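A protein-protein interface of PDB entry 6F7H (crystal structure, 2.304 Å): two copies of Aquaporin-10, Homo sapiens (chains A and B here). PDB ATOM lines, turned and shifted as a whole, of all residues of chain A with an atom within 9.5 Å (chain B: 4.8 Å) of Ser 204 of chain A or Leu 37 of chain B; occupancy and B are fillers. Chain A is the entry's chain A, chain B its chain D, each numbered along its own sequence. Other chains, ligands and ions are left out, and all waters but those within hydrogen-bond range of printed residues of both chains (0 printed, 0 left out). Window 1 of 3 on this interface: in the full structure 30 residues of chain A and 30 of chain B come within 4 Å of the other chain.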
ATOM      1  N   PHE A  55      14.682  14.520 -20.769  1.00  0.00           N
ATOM      2  CA  PHE A  55      14.980  15.886 -21.205  1.00  0.00           C
ATOM      3  C   PHE A  55      13.698  16.694 -21.445  1.00  0.00           C
ATOM      4  O   PHE A  55      13.643  17.882 -21.109  1.00  0.00           O
ATOM      5  CB  PHE A  55      15.860  15.862 -22.480  1.00  0.00           C
ATOM      6  CG  PHE A  55      15.077  15.576 -23.757  1.00  0.00           C
ATOM      7  CD1 PHE A  55      14.491  16.623 -24.485  1.00  0.00           C
ATOM      8  CD2 PHE A  55      14.856  14.258 -24.176  1.00  0.00           C
ATOM      9  CE1 PHE A  55      13.731  16.368 -25.632  1.00  0.00           C
ATOM     10  CE2 PHE A  55      14.102  13.983 -25.323  1.00  0.00           C
ATOM     11  CZ  PHE A  55      13.547  15.033 -26.058  1.00  0.00           C
ATOM     12  N   PHE A  59      12.320  20.102 -19.482  1.00  0.00           N
ATOM     13  CA  PHE A  59      11.995  21.386 -20.100  1.00  0.00           C
ATOM     14  C   PHE A  59      10.552  21.773 -19.791  1.00  0.00           C
ATOM     15  O   PHE A  59      10.268  22.949 -19.509  1.00  0.00           O
ATOM     16  CB  PHE A  59      12.228  21.349 -21.612  1.00  0.00           C
ATOM     17  CG  PHE A  59      13.698  21.369 -22.027  1.00  0.00           C
ATOM     18  CD1 PHE A  59      14.574  22.344 -21.539  1.00  0.00           C
ATOM     19  CD2 PHE A  59      14.188  20.440 -22.945  1.00  0.00           C
ATOM     20  CE1 PHE A  59      15.929  22.370 -21.928  1.00  0.00           C
ATOM     21  CE2 PHE A  59      15.517  20.464 -23.345  1.00  0.00           C
ATOM     22  CZ  PHE A  59      16.396  21.434 -22.829  1.00  0.00           C
ATOM     23  N   TYR A 153      30.700  19.978 -26.019  1.00  0.00           N
ATOM     24  CA  TYR A 153      31.278  20.643 -27.183  1.00  0.00           C
ATOM     25  C   TYR A 153      31.303  22.169 -27.051  1.00  0.00           C
ATOM     26  O   TYR A 153      31.906  22.843 -27.892  1.00  0.00           O
ATOM     27  CB  TYR A 153      30.486  20.251 -28.446  1.00  0.00           C
ATOM     28  CG  TYR A 153      29.022  20.651 -28.357  1.00  0.00           C
ATOM     29  CD1 TYR A 153      28.644  21.970 -28.539  1.00  0.00           C
ATOM     30  CD2 TYR A 153      28.020  19.707 -28.050  1.00  0.00           C
ATOM     31  CE1 TYR A 153      27.303  22.364 -28.437  1.00  0.00           C
ATOM     32  CE2 TYR A 153      26.661  20.083 -27.939  1.00  0.00           C
ATOM     33  CZ  TYR A 153      26.308  21.425 -28.128  1.00  0.00           C
ATOM     34  OH  TYR A 153      24.979  21.858 -28.034  1.00  0.00           O
ATOM     35  N   ASP A 162      24.639  32.170 -26.365  1.00  0.00           N
ATOM     36  CA  ASP A 162      23.401  31.456 -26.170  1.00  0.00           C
ATOM     37  C   ASP A 162      22.501  32.092 -25.115  1.00  0.00           C
ATOM     38  O   ASP A 162      21.330  32.241 -25.332  1.00  0.00           O
ATOM     39  CB  ASP A 162      23.728  29.978 -25.895  1.00  0.00           C
ATOM     40  CG  ASP A 162      22.517  29.118 -25.601  1.00  0.00           C
ATOM     41  OD1 ASP A 162      21.958  28.517 -26.502  1.00  0.00           O
ATOM     42  OD2 ASP A 162      22.162  28.977 -24.446  1.00  0.00           O
ATOM     43  N   LEU A 165      21.309  35.738 -26.022  1.00  0.00           N
ATOM     44  CA  LEU A 165      20.154  35.698 -26.911  1.00  0.00           C
ATOM     45  C   LEU A 165      18.909  35.211 -26.171  1.00  0.00           C
ATOM     46  O   LEU A 165      17.871  35.879 -26.182  1.00  0.00           O
ATOM     47  CB  LEU A 165      20.439  34.801 -28.116  1.00  0.00           C
ATOM     48  CG  LEU A 165      19.205  34.609 -29.009  1.00  0.00           C
ATOM     49  CD1 LEU A 165      18.810  35.934 -29.679  1.00  0.00           C
ATOM     50  CD2 LEU A 165      19.445  33.541 -30.057  1.00  0.00           C
ATOM     51  N   GLY A 166      19.000  34.039 -25.532  1.00  0.00           N
ATOM     52  CA  GLY A 166      17.852  33.497 -24.826  1.00  0.00           C
ATOM     53  C   GLY A 166      17.291  34.458 -23.799  1.00  0.00           C
ATOM     54  O   GLY A 166      16.076  34.662 -23.730  1.00  0.00           O
ATOM     55  N   MET A 169      15.643  37.536 -25.434  1.00  0.00           N
ATOM     56  CA  MET A 169      14.303  37.184 -25.896  1.00  0.00           C
ATOM     57  C   MET A 169      13.331  37.135 -24.726  1.00  0.00           C
ATOM     58  O   MET A 169      12.313  37.839 -24.723  1.00  0.00           O
ATOM     59  CB  MET A 169      14.319  35.856 -26.642  1.00  0.00           C
ATOM     60  CG  MET A 169      14.959  36.016 -28.001  1.00  0.00           C
ATOM     61  SD  MET A 169      15.096  34.488 -28.914  1.00  0.00           S
ATOM     62  CE  MET A 169      13.364  34.195 -29.231  1.00  0.00           C
ATOM     63  N   LEU A 170      13.668  36.365 -23.690  1.00  0.00           N
ATOM     64  CA  LEU A 170      12.821  36.347 -22.505  1.00  0.00           C
ATOM     65  C   LEU A 170      12.466  37.766 -22.051  1.00  0.00           C
ATOM     66  O   LEU A 170      11.286  38.095 -21.885  1.00  0.00           O
ATOM     67  CB  LEU A 170      13.496  35.560 -21.381  1.00  0.00           C
ATOM     68  CG  LEU A 170      12.693  35.538 -20.073  1.00  0.00           C
ATOM     69  CD1 LEU A 170      11.351  34.854 -20.258  1.00  0.00           C
ATOM     70  CD2 LEU A 170      13.502  34.890 -18.989  1.00  0.00           C
ATOM     71  N   MET A 196       4.682  29.298 -21.835  1.00  0.00           N
ATOM     72  CA  MET A 196       4.826  28.918 -23.242  1.00  0.00           C
ATOM     73  C   MET A 196       6.174  29.352 -23.811  1.00  0.00           C
ATOM     74  O   MET A 196       6.833  28.581 -24.529  1.00  0.00           O
ATOM     75  CB  MET A 196       3.678  29.507 -24.065  1.00  0.00           C
ATOM     76  CG  MET A 196       2.317  28.951 -23.603  1.00  0.00           C
ATOM     77  SD  MET A 196       0.841  29.327 -24.605  1.00  0.00           S
ATOM     78  CE  MET A 196       1.085  28.268 -26.048  1.00  0.00           C
ATOM     79  N   LEU A 197       6.594  30.593 -23.523  1.00  0.00           N
ATOM     80  CA  LEU A 197       7.867  31.089 -24.060  1.00  0.00           C
ATOM     81  C   LEU A 197       9.042  30.318 -23.468  1.00  0.00           C
ATOM     82  O   LEU A 197      10.003  29.980 -24.172  1.00  0.00           O
ATOM     83  CB  LEU A 197       8.004  32.592 -23.781  1.00  0.00           C
ATOM     84  CG  LEU A 197       9.255  33.401 -24.177  1.00  0.00           C
ATOM     85  CD1 LEU A 197       9.631  33.257 -25.680  1.00  0.00           C
ATOM     86  CD2 LEU A 197       9.048  34.882 -23.791  1.00  0.00           C
ATOM     87  N   ILE A 198       8.974  30.021 -22.171  1.00  0.00           N
ATOM     88  CA  ILE A 198      10.022  29.234 -21.531  1.00  0.00           C
ATOM     89  C   ILE A 198      10.130  27.870 -22.196  1.00  0.00           C
ATOM     90  O   ILE A 198      11.234  27.375 -22.447  1.00  0.00           O
ATOM     91  CB  ILE A 198       9.735  29.123 -20.021  1.00  0.00           C
ATOM     92  CG1 ILE A 198       9.728  30.541 -19.388  1.00  0.00           C
ATOM     93  CG2 ILE A 198      10.716  28.129 -19.352  1.00  0.00           C
ATOM     94  CD1 ILE A 198      11.149  31.115 -19.082  1.00  0.00           C
ATOM     95  N   LEU A 199       8.981  27.244 -22.492  1.00  0.00           N
ATOM     96  CA  LEU A 199       8.968  25.948 -23.170  1.00  0.00           C
ATOM     97  C   LEU A 199       9.602  26.058 -24.552  1.00  0.00           C
ATOM     98  O   LEU A 199      10.420  25.212 -24.954  1.00  0.00           O
ATOM     99  CB  LEU A 199       7.530  25.445 -23.313  1.00  0.00           C
ATOM    100  CG  LEU A 199       7.201  23.965 -23.158  1.00  0.00           C
ATOM    101  CD1 LEU A 199       5.866  23.516 -23.927  1.00  0.00           C
ATOM    102  CD2 LEU A 199       8.391  23.015 -23.341  1.00  0.00           C
ATOM    103  N   ALA A 200       9.174  27.072 -25.317  1.00  0.00           N
ATOM    104  CA  ALA A 200       9.744  27.316 -26.637  1.00  0.00           C
ATOM    105  C   ALA A 200      11.256  27.513 -26.547  1.00  0.00           C
ATOM    106  O   ALA A 200      12.031  26.865 -27.262  1.00  0.00           O
ATOM    107  CB  ALA A 200       9.051  28.530 -27.265  1.00  0.00           C
ATOM    108  N   LEU A 201      11.705  28.372 -25.644  1.00  0.00           N
ATOM    109  CA  LEU A 201      13.144  28.544 -25.510  1.00  0.00           C
ATOM    110  C   LEU A 201      13.815  27.230 -25.108  1.00  0.00           C
ATOM    111  O   LEU A 201      14.921  26.927 -25.578  1.00  0.00           O
ATOM    112  CB  LEU A 201      13.447  29.664 -24.510  1.00  0.00           C
ATOM    113  CG  LEU A 201      13.055  31.074 -24.972  1.00  0.00           C
ATOM    114  CD1 LEU A 201      13.083  32.102 -23.849  1.00  0.00           C
ATOM    115  CD2 LEU A 201      14.007  31.491 -26.101  1.00  0.00           C
ATOM    116  N   GLY A 202      13.168  26.442 -24.227  1.00  0.00           N
ATOM    117  CA  GLY A 202      13.803  25.223 -23.747  1.00  0.00           C
ATOM    118  C   GLY A 202      14.005  24.202 -24.856  1.00  0.00           C
ATOM    119  O   GLY A 202      15.055  23.546 -24.938  1.00  0.00           O
ATOM    120  N   LEU A 203      13.023  24.102 -25.766  1.00  0.00           N
ATOM    121  CA  LEU A 203      13.027  23.132 -26.846  1.00  0.00           C
ATOM    122  C   LEU A 203      13.788  23.618 -28.078  1.00  0.00           C
ATOM    123  O   LEU A 203      14.152  22.796 -28.921  1.00  0.00           O
ATOM    124  CB  LEU A 203      11.578  22.773 -27.228  1.00  0.00           C
ATOM    125  CG  LEU A 203      10.590  22.191 -26.171  1.00  0.00           C
ATOM    126  CD1 LEU A 203       9.147  22.037 -26.764  1.00  0.00           C
ATOM    127  CD2 LEU A 203      11.065  20.863 -25.581  1.00  0.00           C
ATOM    128  N   SER A 204      14.074  24.918 -28.192  1.00  0.00           N
ATOM    129  CA  SER A 204      14.780  25.471 -29.347  1.00  0.00           C
ATOM    130  C   SER A 204      16.166  25.987 -29.034  1.00  0.00           C
ATOM    131  O   SER A 204      16.986  26.087 -29.954  1.00  0.00           O
ATOM    132  CB  SER A 204      13.982  26.631 -29.955  1.00  0.00           C
ATOM    133  OG  SER A 204      12.724  26.135 -30.408  1.00  0.00           O
ATOM    134  N   MET A 205      16.435  26.346 -27.774  1.00  0.00           N
ATOM    135  CA  MET A 205      17.701  26.942 -27.345  1.00  0.00           C
ATOM    136  C   MET A 205      18.142  26.382 -26.004  1.00  0.00           C
ATOM    137  O   MET A 205      18.800  27.081 -25.224  1.00  0.00           O
ATOM    138  CB  MET A 205      17.609  28.446 -27.197  1.00  0.00           C
ATOM    139  CG  MET A 205      17.123  29.127 -28.398  1.00  0.00           C
ATOM    140  SD  MET A 205      16.981  30.906 -28.125  1.00  0.00           S
ATOM    141  CE  MET A 205      16.116  31.236 -29.645  1.00  0.00           C
ATOM    142  N   GLY A 206      17.784  25.138 -25.715  1.00  0.00           N
ATOM    143  CA  GLY A 206      18.104  24.593 -24.416  1.00  0.00           C
ATOM    144  C   GLY A 206      19.235  23.596 -24.482  1.00  0.00           C
ATOM    145  O   GLY A 206      19.779  23.226 -23.450  1.00  0.00           O
ATOM    146  N   ALA A 207      19.617  23.187 -25.692  1.00  0.00           N
ATOM    147  CA  ALA A 207      20.589  22.106 -25.848  1.00  0.00           C
ATOM    148  C   ALA A 207      22.009  22.515 -25.448  1.00  0.00           C
ATOM    149  O   ALA A 207      22.769  21.682 -24.949  1.00  0.00           O
ATOM    150  CB  ALA A 207      20.578  21.619 -27.291  1.00  0.00           C
ATOM    151  N   ASN A 208      22.413  23.765 -25.720  1.00  0.00           N
ATOM    152  CA  ASN A 208      23.792  24.176 -25.442  1.00  0.00           C
ATOM    153  C   ASN A 208      24.085  24.128 -23.944  1.00  0.00           C
ATOM    154  O   ASN A 208      25.139  23.629 -23.513  1.00  0.00           O
ATOM    155  CB  ASN A 208      24.079  25.592 -25.998  1.00  0.00           C
ATOM    156  CG  ASN A 208      24.193  25.622 -27.519  1.00  0.00           C
ATOM    157  OD1 ASN A 208      24.693  24.680 -28.143  1.00  0.00           O
ATOM    158  ND2 ASN A 208      23.713  26.701 -28.122  1.00  0.00           N
ATOM    159  N   CYS A 209      23.167  24.654 -23.132  1.00  0.00           N
ATOM    160  CA  CYS A 209      23.465  24.691 -21.699  1.00  0.00           C
ATOM    161  C   CYS A 209      22.227  24.834 -20.824  1.00  0.00           C
ATOM    162  O   CYS A 209      22.367  25.295 -19.686  1.00  0.00           O
ATOM    163  CB  CYS A 209      24.440  25.829 -21.407  1.00  0.00           C
ATOM    164  SG  CYS A 209      23.787  27.448 -21.824  1.00  0.00           S
ATOM    165  N   GLY A 210      21.035  24.484 -21.299  1.00  0.00           N
ATOM    166  CA  GLY A 210      19.895  24.370 -20.416  1.00  0.00           C
ATOM    167  C   GLY A 210      19.224  25.654 -19.959  1.00  0.00           C
ATOM    168  O   GLY A 210      18.720  25.690 -18.828  1.00  0.00           O
ATOM    169  N   ILE A 211      19.193  26.693 -20.800  1.00  0.00           N
ATOM    170  CA  ILE A 211      18.466  27.950 -20.553  1.00  0.00           C
ATOM    171  C   ILE A 211      18.360  28.288 -19.066  1.00  0.00           C
ATOM    172  O   ILE A 211      17.252  28.407 -18.522  1.00  0.00           O
ATOM    173  CB  ILE A 211      17.061  27.932 -21.186  1.00  0.00           C
ATOM    174  CG1 ILE A 211      16.259  26.701 -20.740  1.00  0.00           C
ATOM    175  CG2 ILE A 211      17.145  27.998 -22.717  1.00  0.00           C
ATOM    176  CD1 ILE A 211      14.697  26.888 -20.926  1.00  0.00           C
ATOM    177  N   VAL B  33      11.410  35.873 -35.011  1.00  0.00           N
ATOM    178  CA  VAL B  33      11.119  35.051 -33.844  1.00  0.00           C
ATOM    179  C   VAL B  33      10.596  33.676 -34.272  1.00  0.00           C
ATOM    180  O   VAL B  33      11.018  32.640 -33.738  1.00  0.00           O
ATOM    181  CB  VAL B  33      10.107  35.782 -32.935  1.00  0.00           C
ATOM    182  CG1 VAL B  33       9.646  34.862 -31.809  1.00  0.00           C
ATOM    183  CG2 VAL B  33      10.689  37.101 -32.390  1.00  0.00           C
ATOM    184  N   LEU B  34       9.658  33.652 -35.228  1.00  0.00           N
ATOM    185  CA  LEU B  34       9.117  32.394 -35.733  1.00  0.00           C
ATOM    186  C   LEU B  34      10.233  31.458 -36.168  1.00  0.00           C
ATOM    187  O   LEU B  34      10.196  30.248 -35.886  1.00  0.00           O
ATOM    188  CB  LEU B  34       8.185  32.671 -36.912  1.00  0.00           C
ATOM    189  CG  LEU B  34       7.756  31.500 -37.807  1.00  0.00           C
ATOM    190  CD1 LEU B  34       6.633  30.687 -37.139  1.00  0.00           C
ATOM    191  CD2 LEU B  34       7.301  31.983 -39.185  1.00  0.00           C
ATOM    192  N   MET B  35      11.254  32.016 -36.838  1.00  0.00           N
ATOM    193  CA  MET B  35      12.263  31.199 -37.491  1.00  0.00           C
ATOM    194  C   MET B  35      13.353  30.764 -36.518  1.00  0.00           C
ATOM    195  O   MET B  35      13.866  29.648 -36.622  1.00  0.00           O
ATOM    196  CB  MET B  35      12.866  31.969 -38.684  1.00  0.00           C
ATOM    197  CG  MET B  35      11.862  32.202 -39.809  1.00  0.00           C
ATOM    198  SD  MET B  35      11.131  30.671 -40.433  1.00  0.00           S
ATOM    199  CE  MET B  35      12.583  29.622 -40.563  1.00  0.00           C
ATOM    200  N   LEU B  36      13.731  31.635 -35.582  1.00  0.00           N
ATOM    201  CA  LEU B  36      14.681  31.244 -34.551  1.00  0.00           C
ATOM    202  C   LEU B  36      14.157  30.042 -33.766  1.00  0.00           C
ATOM    203  O   LEU B  36      14.852  29.025 -33.603  1.00  0.00           O
ATOM    204  CB  LEU B  36      14.927  32.432 -33.630  1.00  0.00           C
ATOM    205  CG  LEU B  36      16.195  32.580 -32.788  1.00  0.00           C
ATOM    206  CD1 LEU B  36      17.451  32.334 -33.640  1.00  0.00           C
ATOM    207  CD2 LEU B  36      16.212  33.984 -32.222  1.00  0.00           C
ATOM    208  N   LEU B  37      12.910  30.132 -33.296  1.00  0.00           N
ATOM    209  CA  LEU B  37      12.353  29.058 -32.490  1.00  0.00           C
ATOM    210  C   LEU B  37      12.143  27.812 -33.319  1.00  0.00           C
ATOM    211  O   LEU B  37      12.327  26.702 -32.818  1.00  0.00           O
ATOM    212  CB  LEU B  37      11.041  29.504 -31.845  1.00  0.00           C
ATOM    213  CG  LEU B  37      11.214  30.611 -30.808  1.00  0.00           C
ATOM    214  CD1 LEU B  37       9.843  31.123 -30.300  1.00  0.00           C
ATOM    215  CD2 LEU B  37      12.055  30.109 -29.674  1.00  0.00           C
ATOM    216  N   THR B  38      11.783  27.974 -34.592  1.00  0.00           N
ATOM    217  CA  THR B  38      11.462  26.811 -35.405  1.00  0.00           C
ATOM    218  C   THR B  38      12.716  26.046 -35.776  1.00  0.00           C
ATOM    219  O   THR B  38      12.781  24.822 -35.611  1.00  0.00           O
ATOM    220  CB  THR B  38      10.702  27.237 -36.649  1.00  0.00           C
ATOM    221  OG1 THR B  38       9.473  27.847 -36.237  1.00  0.00           O
ATOM    222  CG2 THR B  38      10.409  26.026 -37.532  1.00  0.00           C
ATOM    223  N   GLN B  39      13.734  26.766 -36.256  1.00  0.00           N
ATOM    224  CA  GLN B  39      14.975  26.125 -36.681  1.00  0.00           C
ATOM    225  C   GLN B  39      15.788  25.678 -35.485  1.00  0.00           C
ATOM    226  O   GLN B  39      16.493  24.669 -35.560  1.00  0.00           O
ATOM    227  CB  GLN B  39      15.817  27.088 -37.540  1.00  0.00           C
ATOM    228  CG  GLN B  39      15.127  27.622 -38.792  1.00  0.00           C
ATOM    229  CD  GLN B  39      16.008  28.657 -39.505  1.00  0.00           C
ATOM    230  OE1 GLN B  39      16.627  29.497 -38.856  1.00  0.00           O
ATOM    231  NE2 GLN B  39      16.078  28.583 -40.830  1.00  0.00           N
ATOM    232  N   GLY B  40      15.749  26.457 -34.393  1.00  0.00           N
ATOM    233  CA  GLY B  40      16.469  26.069 -33.191  1.00  0.00           C
ATOM    234  C   GLY B  40      16.073  24.685 -32.712  1.00  0.00           C
ATOM    235  O   GLY B  40      16.933  23.864 -32.368  1.00  0.00           O
ATOM    236  N   ALA B  41      14.763  24.395 -32.718  1.00  0.00           N
ATOM    237  CA  ALA B  41      14.287  23.091 -32.240  1.00  0.00           C
ATOM    238  C   ALA B  41      14.743  21.964 -33.156  1.00  0.00           C
ATOM    239  O   ALA B  41      15.117  20.902 -32.672  1.00  0.00           O
ATOM    240  CB  ALA B  41      12.774  23.098 -32.108  1.00  0.00           C
ATOM    241  N   GLN B  44      18.490  21.577 -32.266  1.00  0.00           N
ATOM    242  CA  GLN B  44      18.564  20.909 -30.963  1.00  0.00           C
ATOM    243  C   GLN B  44      18.374  19.408 -31.093  1.00  0.00           C
ATOM    244  O   GLN B  44      19.161  18.622 -30.547  1.00  0.00           O
ATOM    245  CB  GLN B  44      17.485  21.476 -30.025  1.00  0.00           C
ATOM    246  CG  GLN B  44      17.451  20.915 -28.606  1.00  0.00           C
ATOM    247  CD  GLN B  44      16.956  21.963 -27.612  1.00  0.00           C
ATOM    248  OE1 GLN B  44      17.276  23.174 -27.753  1.00  0.00           O
ATOM    249  NE2 GLN B  44      16.189  21.520 -26.592  1.00  0.00           N
ATOM    250  N   ALA B  61       7.529  22.519 -30.857  1.00  0.00           N
ATOM    251  CA  ALA B  61       8.242  23.805 -30.842  1.00  0.00           C
ATOM    252  C   ALA B  61       7.819  24.685 -32.000  1.00  0.00           C
ATOM    253  O   ALA B  61       7.627  25.893 -31.833  1.00  0.00           O
ATOM    254  CB  ALA B  61       9.754  23.589 -30.877  1.00  0.00           C
ATOM    255  N   ALA B  65       6.306  28.342 -31.685  1.00  0.00           N
ATOM    256  CA  ALA B  65       6.932  29.493 -32.364  1.00  0.00           C
ATOM    257  C   ALA B  65       5.889  30.332 -33.068  1.00  0.00           C
ATOM    258  O   ALA B  65       5.930  31.568 -33.016  1.00  0.00           O
ATOM    259  CB  ALA B  65       7.987  29.021 -33.375  1.00  0.00           C
ATOM    260  N   ILE B  68       3.906  32.307 -30.367  1.00  0.00           N
ATOM    261  CA  ILE B  68       4.683  33.417 -29.829  1.00  0.00           C
ATOM    262  C   ILE B  68       4.894  34.492 -30.890  1.00  0.00           C
ATOM    263  O   ILE B  68       4.754  35.689 -30.614  1.00  0.00           O
ATOM    264  CB  ILE B  68       6.011  32.893 -29.262  1.00  0.00           C
ATOM    265  CG1 ILE B  68       5.716  32.096 -28.005  1.00  0.00           C
ATOM    266  CG2 ILE B  68       7.007  34.080 -28.982  1.00  0.00           C
ATOM    267  CD1 ILE B  68       6.534  30.875 -27.930  1.00  0.00           C
ATOM    268  N   TYR B 122      24.099  27.739 -32.992  1.00  0.00           N
ATOM    269  CA  TYR B 122      24.459  26.323 -32.948  1.00  0.00           C
ATOM    270  C   TYR B 122      25.797  26.015 -33.624  1.00  0.00           C
ATOM    271  O   TYR B 122      26.019  24.875 -34.047  1.00  0.00           O
ATOM    272  CB  TYR B 122      23.338  25.499 -33.580  1.00  0.00           C
ATOM    273  CG  TYR B 122      22.199  25.309 -32.634  1.00  0.00           C
ATOM    274  CD1 TYR B 122      21.170  26.244 -32.546  1.00  0.00           C
ATOM    275  CD2 TYR B 122      22.167  24.192 -31.783  1.00  0.00           C
ATOM    276  CE1 TYR B 122      20.127  26.064 -31.633  1.00  0.00           C
ATOM    277  CE2 TYR B 122      21.119  23.986 -30.887  1.00  0.00           C
ATOM    278  CZ  TYR B 122      20.111  24.925 -30.814  1.00  0.00           C
ATOM    279  OH  TYR B 122      19.124  24.729 -29.896  1.00  0.00           O
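Of chain B, only Leu 37 (2.5 Å), Gly 40 (3.2 Å), Ala 41 (3.5 Å), Gln 44 (3.3 Å), Ala 61 (3.9 Å) and Tyr 122 (2.5 Å) come within 4 Å of Ser 204 of chain A. Leu 37 of chain B touches one residue of chain A. No residue of chain A comes within 4 Å of Thr 38 of chain B. Of the printed residues of chain A, Gly 40 of chain B touches Ser 204 (3.2 Å). Of the printed residues of chain B, Ala 200 of chain A touches Ile 68 (3.5 Å). Printed residues of chain B within 4 Å of Leu 165 of chain A: Leu 36 (3.9 Å). The nearest residue of chain B that does not touch Ser 204 of chain A is Leu 36 of chain B (4.4 Å). The nearest residue of chain A that does not touch Leu 37 of chain B is Ala 200 of chain A (4.04 Å). The nearest printed residue of chain A that does not touch Ile 68 of chain B is Leu 197 of chain A (4.1 Å).
The side-chain hydroxyl of Ser 204 of chain A sits at hydrogen-bond distance from the backbone carbonyl oxygen of Ala 200 of chain A, at 3.3 Å. The backbone carbonyl oxygen (O) of Leu 201 of chain A lies within hydrogen-bond range of the backbone NH (N) of Gly 206 of chain A (3.4 Å). O of Gly 40 of chain B sits at hydrogen-bond distance from OH of Tyr 122 of chain B, at 3.4 Å. OE1 of Gln 44 of chain B lies within hydrogen-bond range of OH of Tyr 122 of chain B, at 3.2 Å.
CE2 of Phe 59 of chain A touches NE2 of Gln 44 of chain B (3.5 Å). Leu 36 of chain B touches Leu 165 of chain A. Met 169 of chain A touches Leu 36 of chain B (SD to CD2, 3.5 Å). CD1 of Ile 68 of chain B touches CB of Ala 200 of chain A, at 3.5 Å. CA of Ala 41 of chain B touches O of Leu 203 of chain A, at 3.3 Å. Ala 41 of chain B touches Ser 204 of chain A. C of Ser 204 of chain A touches OE1 of Gln 44 of chain B, at 3.3 Å. OG of Ser 204 of chain A touches CB of Ala 61 of chain B, at 3.9 Å. CG of Leu 36 of chain B touches CE of Met 205 of chain A, 3.4 Å away. Met 205 of chain A touches Tyr 122 of chain B (CA to OH, 3.7 Å).
No position is printed for both chains. Of the 18 pairs that touch across the chains among the printed residues, none has its exchanged pair printed and touching as well.
The backbone carbonyl oxygen of Gly 202 of chain A is in hydrogen-bond range of the side-chain amide nitrogen of Gln 44 of chain B, 2.9 Å away. NE2 of Gln 44 of chain B lies close to O of Leu 203 of chain A (3.3 Å). OG of Ser 204 of chain A is in hydrogen-bond range of O of Leu 37 of chain B (2.5 Å). The backbone carbonyl oxygen (O) of Ser 204 of chain A lies within hydrogen-bond range of the side-chain hydroxyl (OH) of Tyr 122 of chain B, at 2.5 Å. The side-chain amide oxygen (OE1) of Gln 44 of chain B is in hydrogen-bond range of the backbone NH (N) of Met 205 of chain A. The side-chain amide oxygen of Gln 44 of chain B is in hydrogen-bond range of the backbone NH of Gly 206 of chain A, at 2.9 Å. N of Ala 207 of chain A is in hydrogen-bond range of OE1 of Gln 44 of chain B. The backbone carbonyl oxygen (O) of Ser 204 of chain A lies close to the backbone carbonyl oxygen (O) of Gly 40 of chain B (3.3 Å).
Of the 24 printed residues of chain A, 10 touch a printed residue of chain B. Hydrophobic or aromatic side chains of chain B that line the printed part of chain A: Leu 36, Leu 37, Ala 41, Ala 61, Ile 68 and Tyr 122.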
